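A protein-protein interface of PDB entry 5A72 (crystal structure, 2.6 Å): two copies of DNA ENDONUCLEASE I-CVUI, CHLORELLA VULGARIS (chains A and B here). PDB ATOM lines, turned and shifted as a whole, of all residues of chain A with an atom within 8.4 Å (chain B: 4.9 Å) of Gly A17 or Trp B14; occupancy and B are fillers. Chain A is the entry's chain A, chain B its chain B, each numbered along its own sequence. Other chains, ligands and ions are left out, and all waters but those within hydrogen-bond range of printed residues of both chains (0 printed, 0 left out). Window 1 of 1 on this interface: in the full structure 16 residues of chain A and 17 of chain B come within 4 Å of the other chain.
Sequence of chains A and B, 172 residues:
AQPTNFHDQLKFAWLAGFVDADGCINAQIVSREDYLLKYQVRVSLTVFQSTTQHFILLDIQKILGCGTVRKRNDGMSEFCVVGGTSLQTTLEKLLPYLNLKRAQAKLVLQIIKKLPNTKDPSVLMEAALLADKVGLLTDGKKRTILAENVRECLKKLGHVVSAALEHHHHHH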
ATOM      1  N   GLN A   9     -19.127 -21.197 -19.528  1.00  0.00           N
ATOM      2  CA  GLN A   9     -19.175 -22.307 -18.622  1.00  0.00           C
ATOM      3  C   GLN A   9     -18.139 -23.361 -19.047  1.00  0.00           C
ATOM      4  O   GLN A   9     -17.827 -24.273 -18.285  1.00  0.00           O
ATOM      5  CB  GLN A   9     -20.605 -22.831 -18.591  1.00  0.00           C
ATOM      6  CG  GLN A   9     -21.247 -22.991 -17.203  1.00  0.00           C
ATOM      7  CD  GLN A   9     -21.634 -21.711 -16.436  1.00  0.00           C
ATOM      8  OE1 GLN A   9     -22.345 -20.833 -16.944  1.00  0.00           O
ATOM      9  NE2 GLN A   9     -21.182 -21.630 -15.184  1.00  0.00           N
ATOM     10  N   LEU A  10     -17.595 -23.235 -20.260  1.00  0.00           N
ATOM     11  CA  LEU A  10     -16.399 -24.007 -20.625  1.00  0.00           C
ATOM     12  C   LEU A  10     -15.174 -23.448 -19.896  1.00  0.00           C
ATOM     13  O   LEU A  10     -14.296 -24.190 -19.452  1.00  0.00           O
ATOM     14  CB  LEU A  10     -16.167 -23.997 -22.132  1.00  0.00           C
ATOM     15  CG  LEU A  10     -16.951 -25.051 -22.909  1.00  0.00           C
ATOM     16  CD1 LEU A  10     -16.984 -24.723 -24.388  1.00  0.00           C
ATOM     17  CD2 LEU A  10     -16.336 -26.419 -22.692  1.00  0.00           C
ATOM     18  N   LYS A  11     -15.129 -22.128 -19.777  1.00  0.00           N
ATOM     19  CA  LYS A  11     -14.116 -21.471 -18.967  1.00  0.00           C
ATOM     20  C   LYS A  11     -14.204 -21.931 -17.505  1.00  0.00           C
ATOM     21  O   LYS A  11     -13.203 -22.342 -16.925  1.00  0.00           O
ATOM     22  CB  LYS A  11     -14.249 -19.944 -19.071  1.00  0.00           C
ATOM     23  CG  LYS A  11     -13.875 -19.380 -20.431  1.00  0.00           C
ATOM     24  CD  LYS A  11     -12.529 -19.962 -20.879  1.00  0.00           C
ATOM     25  CE  LYS A  11     -12.039 -19.393 -22.214  1.00  0.00           C
ATOM     26  NZ  LYS A  11     -11.413 -18.049 -22.047  1.00  0.00           N
ATOM     27  N   PHE A  12     -15.398 -21.882 -16.919  1.00  0.00           N
ATOM     28  CA  PHE A  12     -15.585 -22.253 -15.514  1.00  0.00           C
ATOM     29  C   PHE A  12     -15.280 -23.737 -15.267  1.00  0.00           C
ATOM     30  O   PHE A  12     -14.661 -24.100 -14.257  1.00  0.00           O
ATOM     31  CB  PHE A  12     -17.017 -21.908 -15.062  1.00  0.00           C
ATOM     32  CG  PHE A  12     -17.284 -20.432 -14.994  1.00  0.00           C
ATOM     33  CD1 PHE A  12     -16.326 -19.575 -14.475  1.00  0.00           C
ATOM     34  CD2 PHE A  12     -18.465 -19.904 -15.463  1.00  0.00           C
ATOM     35  CE1 PHE A  12     -16.554 -18.223 -14.411  1.00  0.00           C
ATOM     36  CE2 PHE A  12     -18.704 -18.547 -15.431  1.00  0.00           C
ATOM     37  CZ  PHE A  12     -17.753 -17.699 -14.901  1.00  0.00           C
ATOM     38  N   ALA A  13     -15.676 -24.584 -16.210  1.00  0.00           N
ATOM     39  CA  ALA A  13     -15.387 -26.003 -16.091  1.00  0.00           C
ATOM     40  C   ALA A  13     -13.878 -26.239 -16.090  1.00  0.00           C
ATOM     41  O   ALA A  13     -13.372 -26.998 -15.258  1.00  0.00           O
ATOM     42  CB  ALA A  13     -16.058 -26.773 -17.195  1.00  0.00           C
ATOM     43  N   TRP A  14     -13.166 -25.559 -16.992  1.00  0.00           N
ATOM     44  CA  TRP A  14     -11.707 -25.583 -17.004  1.00  0.00           C
ATOM     45  C   TRP A  14     -11.148 -25.078 -15.689  1.00  0.00           C
ATOM     46  O   TRP A  14     -10.281 -25.712 -15.093  1.00  0.00           O
ATOM     47  CB  TRP A  14     -11.133 -24.738 -18.146  1.00  0.00           C
ATOM     48  CG  TRP A  14      -9.618 -24.684 -18.089  1.00  0.00           C
ATOM     49  CD1 TRP A  14      -8.740 -25.556 -18.668  1.00  0.00           C
ATOM     50  CD2 TRP A  14      -8.820 -23.727 -17.378  1.00  0.00           C
ATOM     51  NE1 TRP A  14      -7.450 -25.193 -18.370  1.00  0.00           N
ATOM     52  CE2 TRP A  14      -7.472 -24.077 -17.579  1.00  0.00           C
ATOM     53  CE3 TRP A  14      -9.119 -22.607 -16.589  1.00  0.00           C
ATOM     54  CZ2 TRP A  14      -6.425 -23.349 -17.026  1.00  0.00           C
ATOM     55  CZ3 TRP A  14      -8.079 -21.885 -16.044  1.00  0.00           C
ATOM     56  CH2 TRP A  14      -6.746 -22.259 -16.267  1.00  0.00           C
ATOM     57  N   LEU A  15     -11.640 -23.925 -15.243  1.00  0.00           N
ATOM     58  CA  LEU A  15     -11.219 -23.365 -13.963  1.00  0.00           C
ATOM     59  C   LEU A  15     -11.494 -24.327 -12.795  1.00  0.00           C
ATOM     60  O   LEU A  15     -10.635 -24.534 -11.924  1.00  0.00           O
ATOM     61  CB  LEU A  15     -11.908 -22.030 -13.715  1.00  0.00           C
ATOM     62  CG  LEU A  15     -11.400 -21.285 -12.475  1.00  0.00           C
ATOM     63  CD1 LEU A  15      -9.883 -21.393 -12.354  1.00  0.00           C
ATOM     64  CD2 LEU A  15     -11.806 -19.827 -12.526  1.00  0.00           C
ATOM     65  N   ALA A  16     -12.677 -24.927 -12.783  1.00  0.00           N
ATOM     66  CA  ALA A  16     -12.978 -25.904 -11.749  1.00  0.00           C
ATOM     67  C   ALA A  16     -11.938 -27.015 -11.718  1.00  0.00           C
ATOM     68  O   ALA A  16     -11.486 -27.417 -10.642  1.00  0.00           O
ATOM     69  CB  ALA A  16     -14.350 -26.486 -11.952  1.00  0.00           C
ATOM     70  N   GLY A  17     -11.561 -27.500 -12.905  1.00  0.00           N
ATOM     71  CA  GLY A  17     -10.567 -28.551 -13.016  1.00  0.00           C
ATOM     72  C   GLY A  17      -9.231 -28.066 -12.493  1.00  0.00           C
ATOM     73  O   GLY A  17      -8.496 -28.802 -11.832  1.00  0.00           O
ATOM     74  N   PHE A  18      -8.925 -26.804 -12.769  1.00  0.00           N
ATOM     75  CA  PHE A  18      -7.675 -26.230 -12.312  1.00  0.00           C
ATOM     76  C   PHE A  18      -7.676 -26.015 -10.803  1.00  0.00           C
ATOM     77  O   PHE A  18      -6.687 -26.317 -10.132  1.00  0.00           O
ATOM     78  CB  PHE A  18      -7.396 -24.917 -13.034  1.00  0.00           C
ATOM     79  CG  PHE A  18      -5.959 -24.530 -13.023  1.00  0.00           C
ATOM     80  CD1 PHE A  18      -5.082 -25.067 -13.955  1.00  0.00           C
ATOM     81  CD2 PHE A  18      -5.468 -23.639 -12.080  1.00  0.00           C
ATOM     82  CE1 PHE A  18      -3.731 -24.708 -13.954  1.00  0.00           C
ATOM     83  CE2 PHE A  18      -4.123 -23.275 -12.068  1.00  0.00           C
ATOM     84  CZ  PHE A  18      -3.252 -23.808 -13.003  1.00  0.00           C
ATOM     85  N   VAL A  19      -8.778 -25.499 -10.263  1.00  0.00           N
ATOM     86  CA  VAL A  19      -8.883 -25.345  -8.812  1.00  0.00           C
ATOM     87  C   VAL A  19      -8.868 -26.723  -8.135  1.00  0.00           C
ATOM     88  O   VAL A  19      -8.220 -26.906  -7.102  1.00  0.00           O
ATOM     89  CB  VAL A  19     -10.164 -24.585  -8.389  1.00  0.00           C
ATOM     90  CG1 VAL A  19     -10.178 -24.362  -6.897  1.00  0.00           C
ATOM     91  CG2 VAL A  19     -10.248 -23.271  -9.090  1.00  0.00           C
ATOM     92  N   ASP A  20      -9.572 -27.696  -8.713  1.00  0.00           N
ATOM     93  CA  ASP A  20      -9.597 -29.029  -8.128  1.00  0.00           C
ATOM     94  C   ASP A  20      -8.185 -29.564  -7.938  1.00  0.00           C
ATOM     95  O   ASP A  20      -7.901 -30.289  -6.989  1.00  0.00           O
ATOM     96  CB  ASP A  20     -10.396 -29.996  -8.998  1.00  0.00           C
ATOM     97  CG  ASP A  20     -11.823 -30.162  -8.529  1.00  0.00           C
ATOM     98  OD1 ASP A  20     -12.090 -29.918  -7.330  1.00  0.00           O
ATOM     99  OD2 ASP A  20     -12.680 -30.548  -9.360  1.00  0.00           O
ATOM    100  N   ALA A  21      -7.291 -29.186  -8.839  1.00  0.00           N
ATOM    101  CA  ALA A  21      -5.964 -29.756  -8.832  1.00  0.00           C
ATOM    102  C   ALA A  21      -4.960 -28.877  -8.083  1.00  0.00           C
ATOM    103  O   ALA A  21      -4.359 -29.322  -7.108  1.00  0.00           O
ATOM    104  CB  ALA A  21      -5.509 -30.006 -10.258  1.00  0.00           C
ATOM    105  N   ASP A  22      -4.784 -27.636  -8.536  1.00  0.00           N
ATOM    106  CA  ASP A  22      -3.751 -26.750  -7.992  1.00  0.00           C
ATOM    107  C   ASP A  22      -4.330 -25.642  -7.134  1.00  0.00           C
ATOM    108  O   ASP A  22      -3.724 -24.574  -7.007  1.00  0.00           O
ATOM    109  CB  ASP A  22      -2.929 -26.112  -9.118  1.00  0.00           C
ATOM    110  CG  ASP A  22      -1.704 -26.929  -9.485  1.00  0.00           C
ATOM    111  OD1 ASP A  22      -1.612 -28.092  -9.037  1.00  0.00           O
ATOM    112  OD2 ASP A  22      -0.837 -26.413 -10.231  1.00  0.00           O
ATOM    113  N   GLY A  23      -5.502 -25.889  -6.558  1.00  0.00           N
ATOM    114  CA  GLY A  23      -6.212 -24.855  -5.837  1.00  0.00           C
ATOM    115  C   GLY A  23      -6.413 -25.161  -4.372  1.00  0.00           C
ATOM    116  O   GLY A  23      -5.928 -26.158  -3.836  1.00  0.00           O
ATOM    117  N   LEU A  94     -18.290 -22.076  -9.959  1.00  0.00           N
ATOM    118  CA  LEU A  94     -17.487 -23.286 -10.082  1.00  0.00           C
ATOM    119  C   LEU A  94     -18.221 -24.521  -9.595  1.00  0.00           C
ATOM    120  O   LEU A  94     -17.992 -25.615 -10.097  1.00  0.00           O
ATOM    121  CB  LEU A  94     -16.179 -23.148  -9.309  1.00  0.00           C
ATOM    122  CG  LEU A  94     -15.332 -21.931  -9.664  1.00  0.00           C
ATOM    123  CD1 LEU A  94     -14.036 -21.975  -8.888  1.00  0.00           C
ATOM    124  CD2 LEU A  94     -15.061 -21.895 -11.157  1.00  0.00           C
ATOM    125  N   PRO A  96     -20.985 -26.232  -9.944  1.00  0.00           N
ATOM    126  CA  PRO A  96     -21.441 -27.331 -10.811  1.00  0.00           C
ATOM    127  C   PRO A  96     -20.322 -28.233 -11.341  1.00  0.00           C
ATOM    128  O   PRO A  96     -20.603 -29.360 -11.739  1.00  0.00           O
ATOM    129  CB  PRO A  96     -22.107 -26.604 -11.990  1.00  0.00           C
ATOM    130  CG  PRO A  96     -22.398 -25.233 -11.500  1.00  0.00           C
ATOM    131  CD  PRO A  96     -21.334 -24.913 -10.510  1.00  0.00           C
ATOM    132  N   TYR A  97     -19.083 -27.746 -11.337  1.00  0.00           N
ATOM    133  CA  TYR A  97     -17.969 -28.407 -12.028  1.00  0.00           C
ATOM    134  C   TYR A  97     -16.883 -28.919 -11.100  1.00  0.00           C
ATOM    135  O   TYR A  97     -16.051 -29.728 -11.499  1.00  0.00           O
ATOM    136  CB  TYR A  97     -17.354 -27.454 -13.047  1.00  0.00           C
ATOM    137  CG  TYR A  97     -18.396 -26.911 -13.945  1.00  0.00           C
ATOM    138  CD1 TYR A  97     -19.154 -27.772 -14.693  1.00  0.00           C
ATOM    139  CD2 TYR A  97     -18.667 -25.555 -14.017  1.00  0.00           C
ATOM    140  CE1 TYR A  97     -20.130 -27.321 -15.510  1.00  0.00           C
ATOM    141  CE2 TYR A  97     -19.663 -25.086 -14.850  1.00  0.00           C
ATOM    142  CZ  TYR A  97     -20.381 -25.993 -15.591  1.00  0.00           C
ATOM    143  OH  TYR A  97     -21.382 -25.633 -16.430  1.00  0.00           O
ATOM    144  N   LEU A  98     -16.881 -28.457  -9.862  1.00  0.00           N
ATOM    145  CA  LEU A  98     -15.898 -28.966  -8.925  1.00  0.00           C
ATOM    146  C   LEU A  98     -16.172 -30.442  -8.682  1.00  0.00           C
ATOM    147  O   LEU A  98     -17.324 -30.872  -8.655  1.00  0.00           O
ATOM    148  CB  LEU A  98     -15.926 -28.180  -7.615  1.00  0.00           C
ATOM    149  CG  LEU A  98     -15.512 -26.708  -7.700  1.00  0.00           C
ATOM    150  CD1 LEU A  98     -15.580 -26.095  -6.320  1.00  0.00           C
ATOM    151  CD2 LEU A  98     -14.126 -26.530  -8.265  1.00  0.00           C
ATOM    152  N   ASN A  99     -15.112 -31.227  -8.550  1.00  0.00           N
ATOM    153  CA  ASN A  99     -15.273 -32.616  -8.165  1.00  0.00           C
ATOM    154  C   ASN A  99     -14.568 -32.892  -6.842  1.00  0.00           C
ATOM    155  O   ASN A  99     -15.239 -33.154  -5.834  1.00  0.00           O
ATOM    156  CB  ASN A  99     -14.785 -33.537  -9.276  1.00  0.00           C
ATOM    157  CG  ASN A  99     -15.713 -33.512 -10.496  1.00  0.00           C
ATOM    158  OD1 ASN A  99     -16.807 -34.097 -10.492  1.00  0.00           O
ATOM    159  ND2 ASN A  99     -15.280 -32.824 -11.543  1.00  0.00           N
ATOM    160  N   LEU A 100     -13.241 -32.795  -6.815  1.00  0.00           N
ATOM    161  CA  LEU A 100     -12.502 -32.984  -5.560  1.00  0.00           C
ATOM    162  C   LEU A 100     -12.897 -32.046  -4.423  1.00  0.00           C
ATOM    163  O   LEU A 100     -12.873 -32.434  -3.255  1.00  0.00           O
ATOM    164  CB  LEU A 100     -11.012 -32.823  -5.787  1.00  0.00           C
ATOM    165  CG  LEU A 100     -10.451 -33.839  -6.758  1.00  0.00           C
ATOM    166  CD1 LEU A 100      -8.936 -33.701  -6.810  1.00  0.00           C
ATOM    167  CD2 LEU A 100     -10.874 -35.225  -6.321  1.00  0.00           C
ATOM    168  N   LYS A 101     -13.256 -30.815  -4.752  1.00  0.00           N
ATOM    169  CA  LYS A 101     -13.381 -29.801  -3.714  1.00  0.00           C
ATOM    170  C   LYS A 101     -14.805 -29.295  -3.525  1.00  0.00           C
ATOM    171  O   LYS A 101     -15.006 -28.225  -2.962  1.00  0.00           O
ATOM    172  CB  LYS A 101     -12.432 -28.626  -4.020  1.00  0.00           C
ATOM    173  CG  LYS A 101     -11.132 -28.705  -3.248  1.00  0.00           C
ATOM    174  CD  LYS A 101      -9.906 -28.325  -4.057  1.00  0.00           C
ATOM    175  CE  LYS A 101      -8.637 -28.757  -3.303  1.00  0.00           C
ATOM    176  NZ  LYS A 101      -7.334 -28.533  -4.022  1.00  0.00           N
ATOM    177  N   ARG A 102     -15.797 -30.051  -3.977  1.00  0.00           N
ATOM    178  CA  ARG A 102     -17.159 -29.551  -3.874  1.00  0.00           C
ATOM    179  C   ARG A 102     -17.595 -29.490  -2.409  1.00  0.00           C
ATOM    180  O   ARG A 102     -18.414 -28.650  -2.022  1.00  0.00           O
ATOM    181  CB  ARG A 102     -18.131 -30.402  -4.689  1.00  0.00           C
ATOM    182  CG  ARG A 102     -19.490 -29.736  -4.860  1.00  0.00           C
ATOM    183  CD  ARG A 102     -20.460 -30.613  -5.619  1.00  0.00           C
ATOM    184  NE  ARG A 102     -20.069 -30.765  -7.011  1.00  0.00           N
ATOM    185  CZ  ARG A 102     -20.629 -31.624  -7.861  1.00  0.00           C
ATOM    186  NH1 ARG A 102     -21.611 -32.428  -7.454  1.00  0.00           N
ATOM    187  NH2 ARG A 102     -20.200 -31.684  -9.123  1.00  0.00           N
ATOM    188  N   LEU B  10     -17.756 -30.344 -21.629  1.00  0.00           N
ATOM    189  CA  LEU B  10     -17.605 -29.829 -20.276  1.00  0.00           C
ATOM    190  C   LEU B  10     -16.674 -30.728 -19.470  1.00  0.00           C
ATOM    191  O   LEU B  10     -15.826 -30.248 -18.718  1.00  0.00           O
ATOM    192  CB  LEU B  10     -18.961 -29.697 -19.595  1.00  0.00           C
ATOM    193  CG  LEU B  10     -19.681 -28.381 -19.879  1.00  0.00           C
ATOM    194  CD1 LEU B  10     -20.909 -28.255 -19.018  1.00  0.00           C
ATOM    195  CD2 LEU B  10     -18.755 -27.216 -19.616  1.00  0.00           C
ATOM    196  N   LYS B  11     -16.822 -32.032 -19.643  1.00  0.00           N
ATOM    197  CA  LYS B  11     -15.902 -32.976 -19.030  1.00  0.00           C
ATOM    198  C   LYS B  11     -14.467 -32.733 -19.512  1.00  0.00           C
ATOM    199  O   LYS B  11     -13.545 -32.648 -18.700  1.00  0.00           O
ATOM    200  CB  LYS B  11     -16.337 -34.417 -19.331  1.00  0.00           C
ATOM    201  CG  LYS B  11     -17.602 -34.840 -18.592  1.00  0.00           C
ATOM    202  CD  LYS B  11     -17.387 -34.758 -17.076  1.00  0.00           C
ATOM    203  CE  LYS B  11     -18.521 -35.410 -16.288  1.00  0.00           C
ATOM    204  NZ  LYS B  11     -19.807 -34.682 -16.480  1.00  0.00           N
ATOM    205  N   PHE B  12     -14.275 -32.609 -20.825  1.00  0.00           N
ATOM    206  CA  PHE B  12     -12.925 -32.450 -21.376  1.00  0.00           C
ATOM    207  C   PHE B  12     -12.298 -31.160 -20.895  1.00  0.00           C
ATOM    208  O   PHE B  12     -11.105 -31.113 -20.580  1.00  0.00           O
ATOM    209  CB  PHE B  12     -12.939 -32.481 -22.907  1.00  0.00           C
ATOM    210  CG  PHE B  12     -13.297 -33.819 -23.486  1.00  0.00           C
ATOM    211  CD1 PHE B  12     -13.003 -34.986 -22.798  1.00  0.00           C
ATOM    212  CD2 PHE B  12     -13.935 -33.909 -24.713  1.00  0.00           C
ATOM    213  CE1 PHE B  12     -13.338 -36.218 -23.315  1.00  0.00           C
ATOM    214  CE2 PHE B  12     -14.276 -35.137 -25.237  1.00  0.00           C
ATOM    215  CZ  PHE B  12     -13.978 -36.296 -24.532  1.00  0.00           C
ATOM    216  N   ALA B  13     -13.117 -30.111 -20.841  1.00  0.00           N
ATOM    217  CA  ALA B  13     -12.658 -28.814 -20.359  1.00  0.00           C
ATOM    218  C   ALA B  13     -12.217 -28.940 -18.907  1.00  0.00           C
ATOM    219  O   ALA B  13     -11.160 -28.437 -18.532  1.00  0.00           O
ATOM    220  CB  ALA B  13     -13.745 -27.764 -20.507  1.00  0.00           C
ATOM    221  N   TRP B  14     -13.017 -29.629 -18.099  1.00  0.00           N
ATOM    222  CA  TRP B  14     -12.666 -29.840 -16.707  1.00  0.00           C
ATOM    223  C   TRP B  14     -11.357 -30.585 -16.625  1.00  0.00           C
ATOM    224  O   TRP B  14     -10.445 -30.176 -15.912  1.00  0.00           O
ATOM    225  CB  TRP B  14     -13.751 -30.623 -15.960  1.00  0.00           C
ATOM    226  CG  TRP B  14     -13.342 -30.936 -14.539  1.00  0.00           C
ATOM    227  CD1 TRP B  14     -13.557 -30.164 -13.429  1.00  0.00           C
ATOM    228  CD2 TRP B  14     -12.625 -32.090 -14.089  1.00  0.00           C
ATOM    229  NE1 TRP B  14     -13.019 -30.771 -12.323  1.00  0.00           N
ATOM    230  CE2 TRP B  14     -12.441 -31.952 -12.702  1.00  0.00           C
ATOM    231  CE3 TRP B  14     -12.120 -33.225 -14.727  1.00  0.00           C
ATOM    232  CZ2 TRP B  14     -11.776 -32.904 -11.946  1.00  0.00           C
ATOM    233  CZ3 TRP B  14     -11.465 -34.166 -13.975  1.00  0.00           C
ATOM    234  CH2 TRP B  14     -11.299 -34.001 -12.594  1.00  0.00           C
ATOM    235  N   LEU B  15     -11.281 -31.691 -17.362  1.00  0.00           N
ATOM    236  CA  LEU B  15     -10.082 -32.514 -17.400  1.00  0.00           C
ATOM    237  C   LEU B  15      -8.849 -31.698 -17.848  1.00  0.00           C
ATOM    238  O   LEU B  15      -7.786 -31.763 -17.218  1.00  0.00           O
ATOM    239  CB  LEU B  15     -10.313 -33.717 -18.315  1.00  0.00           C
ATOM    240  CG  LEU B  15      -9.243 -34.805 -18.273  1.00  0.00           C
ATOM    241  CD1 LEU B  15      -8.758 -35.037 -16.856  1.00  0.00           C
ATOM    242  CD2 LEU B  15      -9.793 -36.089 -18.834  1.00  0.00           C
ATOM    243  N   ALA B  16      -9.001 -30.916 -18.913  1.00  0.00           N
ATOM    244  CA  ALA B  16      -7.933 -30.019 -19.342  1.00  0.00           C
ATOM    245  C   ALA B  16      -7.409 -29.145 -18.198  1.00  0.00           C
ATOM    246  O   ALA B  16      -6.195 -28.938 -18.069  1.00  0.00           O
ATOM    247  CB  ALA B  16      -8.410 -29.138 -20.485  1.00  0.00           C
ATOM    248  N   GLY B  17      -8.334 -28.630 -17.385  1.00  0.00           N
ATOM    249  CA  GLY B  17      -7.972 -27.823 -16.234  1.00  0.00           C
ATOM    250  C   GLY B  17      -7.180 -28.657 -15.251  1.00  0.00           C
ATOM    251  O   GLY B  17      -6.154 -28.230 -14.723  1.00  0.00           O
ATOM    252  N   PHE B  18      -7.642 -29.879 -15.037  1.00  0.00           N
ATOM    253  CA  PHE B  18      -6.991 -30.765 -14.096  1.00  0.00           C
ATOM    254  C   PHE B  18      -5.607 -31.168 -14.578  1.00  0.00           C
ATOM    255  O   PHE B  18      -4.663 -31.182 -13.797  1.00  0.00           O
ATOM    256  CB  PHE B  18      -7.846 -32.001 -13.846  1.00  0.00           C
ATOM    257  CG  PHE B  18      -7.531 -32.687 -12.558  1.00  0.00           C
ATOM    258  CD1 PHE B  18      -8.113 -32.255 -11.369  1.00  0.00           C
ATOM    259  CD2 PHE B  18      -6.643 -33.750 -12.521  1.00  0.00           C
ATOM    260  CE1 PHE B  18      -7.826 -32.886 -10.160  1.00  0.00           C
ATOM    261  CE2 PHE B  18      -6.347 -34.382 -11.319  1.00  0.00           C
ATOM    262  CZ  PHE B  18      -6.941 -33.954 -10.135  1.00  0.00           C
ATOM    263  N   ILE B  56     -10.700 -40.531  -8.219  1.00  0.00           N
ATOM    264  CA  ILE B  56     -10.845 -39.490  -9.242  1.00  0.00           C
ATOM    265  C   ILE B  56     -10.055 -39.904 -10.503  1.00  0.00           C
ATOM    266  O   ILE B  56     -10.469 -39.642 -11.636  1.00  0.00           O
ATOM    267  CB  ILE B  56     -10.399 -38.080  -8.714  1.00  0.00           C
ATOM    268  CG1 ILE B  56     -10.868 -36.970  -9.650  1.00  0.00           C
ATOM    269  CG2 ILE B  56      -8.898 -37.980  -8.506  1.00  0.00           C
ATOM    270  CD1 ILE B  56     -12.361 -36.870  -9.762  1.00  0.00           C
ATOM    271  N   ILE B  60     -11.359 -40.275 -14.452  1.00  0.00           N
ATOM    272  CA  ILE B  60     -10.700 -39.737 -15.637  1.00  0.00           C
ATOM    273  C   ILE B  60     -10.608 -40.817 -16.717  1.00  0.00           C
ATOM    274  O   ILE B  60     -10.986 -40.596 -17.858  1.00  0.00           O
ATOM    275  CB  ILE B  60      -9.311 -39.161 -15.276  1.00  0.00           C
ATOM    276  CG1 ILE B  60      -9.511 -37.866 -14.472  1.00  0.00           C
ATOM    277  CG2 ILE B  60      -8.472 -38.911 -16.530  1.00  0.00           C
ATOM    278  CD1 ILE B  60      -8.291 -37.334 -13.792  1.00  0.00           C
ATOM    279  N   ILE B  63     -13.829 -41.272 -18.367  1.00  0.00           N
ATOM    280  CA  ILE B  63     -14.040 -40.165 -19.295  1.00  0.00           C
ATOM    281  C   ILE B  63     -13.310 -40.375 -20.619  1.00  0.00           C
ATOM    282  O   ILE B  63     -13.845 -40.090 -21.688  1.00  0.00           O
ATOM    283  CB  ILE B  63     -13.570 -38.835 -18.681  1.00  0.00           C
ATOM    284  CG1 ILE B  63     -14.511 -38.393 -17.570  1.00  0.00           C
ATOM    285  CG2 ILE B  63     -13.525 -37.740 -19.718  1.00  0.00           C
ATOM    286  CD1 ILE B  63     -14.006 -37.202 -16.826  1.00  0.00           C
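Leu B10 touches its own counterpart, Leu A10.
Leu A10 touches Ala B13, and with the chains exchanged Ala A13 touches Leu B10.
Gly A17 touches its own counterpart, Gly B17.
Gly A17 touches Phe B18, and with the chains exchanged Phe A18 touches Gly B17.
Positions printed for both chains: 10, 11, 12, 13, 14, 15, 16, 17 and 18.
Of the 21 pairs that touch across the chains among the printed residues, 12 have their exchanged pair printed and touching as well.
The backbone NH of Asn A99 is in hydrogen-bond range of the side-chain carboxylate of Asp A20 (2.7 Å).
OD1 of Asp A20 lies within hydrogen-bond range of N of Leu A100 (3.1 Å).
The side-chain carboxylate of Asp A20 is in hydrogen-bond range of the backbone NH of Lys A101 (3.0 Å).
The side-chain amide nitrogen (ND2) of Asn A99 is in hydrogen-bond range of the backbone carbonyl oxygen (O) of Tyr A97.
Gln A9 touches Leu B10 (O to CD2, 3.4 Å).
Leu A10 touches Leu B10.
Leu B10 touches Ala A13 (CD2 to CB, 3.7 Å).
Ala B13 touches Trp A14.
Gly B17 touches Trp A14.
O of Trp B14 touches CA of Gly A17, 3.3 Å away.
C of Gly A17 touches C of Gly B17, 3.5 Å away.
CB of Asp A20 touches CD1 of Phe B18 (3.99 Å).
CD1 of Leu B10 touches CE1 of Tyr A97, 3.7 Å away.
CB of Ile B56 touches CD2 of Leu A100, 3.8 Å away.
Of the printed residues of chain B, Leu A10 touches Leu B10 and Ala B13.
Leu A15 touches none of the printed residues of chain B.
Gly A17 touches just these residues of chain B: Trp B14 (3.3 Å), Gly B17 (3.5 Å) and Phe B18 (3.4 Å).
Of the printed residues of chain B, Phe A18 touches Gly B17.
Printed residues of chain B within 4 Å of Asp A20: Trp B14 (3.0 Å) and Phe B18 (3.99 Å).
Of the printed residues of chain B, Ala A21 touches Phe B18.
Lys B11 touches none of the printed residues of chain A.
Of chain A, only Leu A10 (3.6 Å) and Trp A14 (3.3 Å) come within 4 Å of Ala B13.
Of chain A, only Ala A13 (3.3 Å), Ala A16 (3.9 Å), Gly A17 (3.3 Å), Asp A20 (3.0 Å), Tyr A97 (3.2 Å) and Asn A99 (3.2 Å) come within 4 Å of Trp B14.
Printed residues of chain A within 4 Å of Ala B16: Trp A14.
Gly B17 touches just these residues of chain A: Trp A14, Gly A17 and Phe A18.
The nearest printed residue of chain B that does not touch Gly A17 is Leu B15 (5.4 Å).
The nearest residue of chain A that does not touch Trp B14 is Trp A14 (4.2 Å).
Of the 12 printed residues of chain B, 7 touch a printed residue of chain A.
Printed residues of chain B that touch a printed residue of chain A: Leu B10, Ala B13, Trp B14, Ala B16, Gly B17, Phe B18 and Ile B56.
Hydrophobic or aromatic side chains of chain A within 4 Å of the printed part of chain B: Leu A10, Ala A13, Trp A14, Phe A18, Ala A21, Tyr A97 and Leu A100.
Among the printed residues, no Asp or Glu carboxylate lies within 4 Å of a Lys or Arg side-chain nitrogen of the other chain.
O of Gly A17 lies close to N of Phe B18, 3.5 Å away.
The side-chain carboxylate (OD2) of Asp A20 sits at hydrogen-bond distance from the indole nitrogen (NE1) of Trp B14 (3.0 Å).
The backbone carbonyl oxygen of Tyr A97 sits close to the indole nitrogen of Trp B14.
ND2 of Asn A99 lies close to NE1 of Trp B14, at 3.2 Å.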
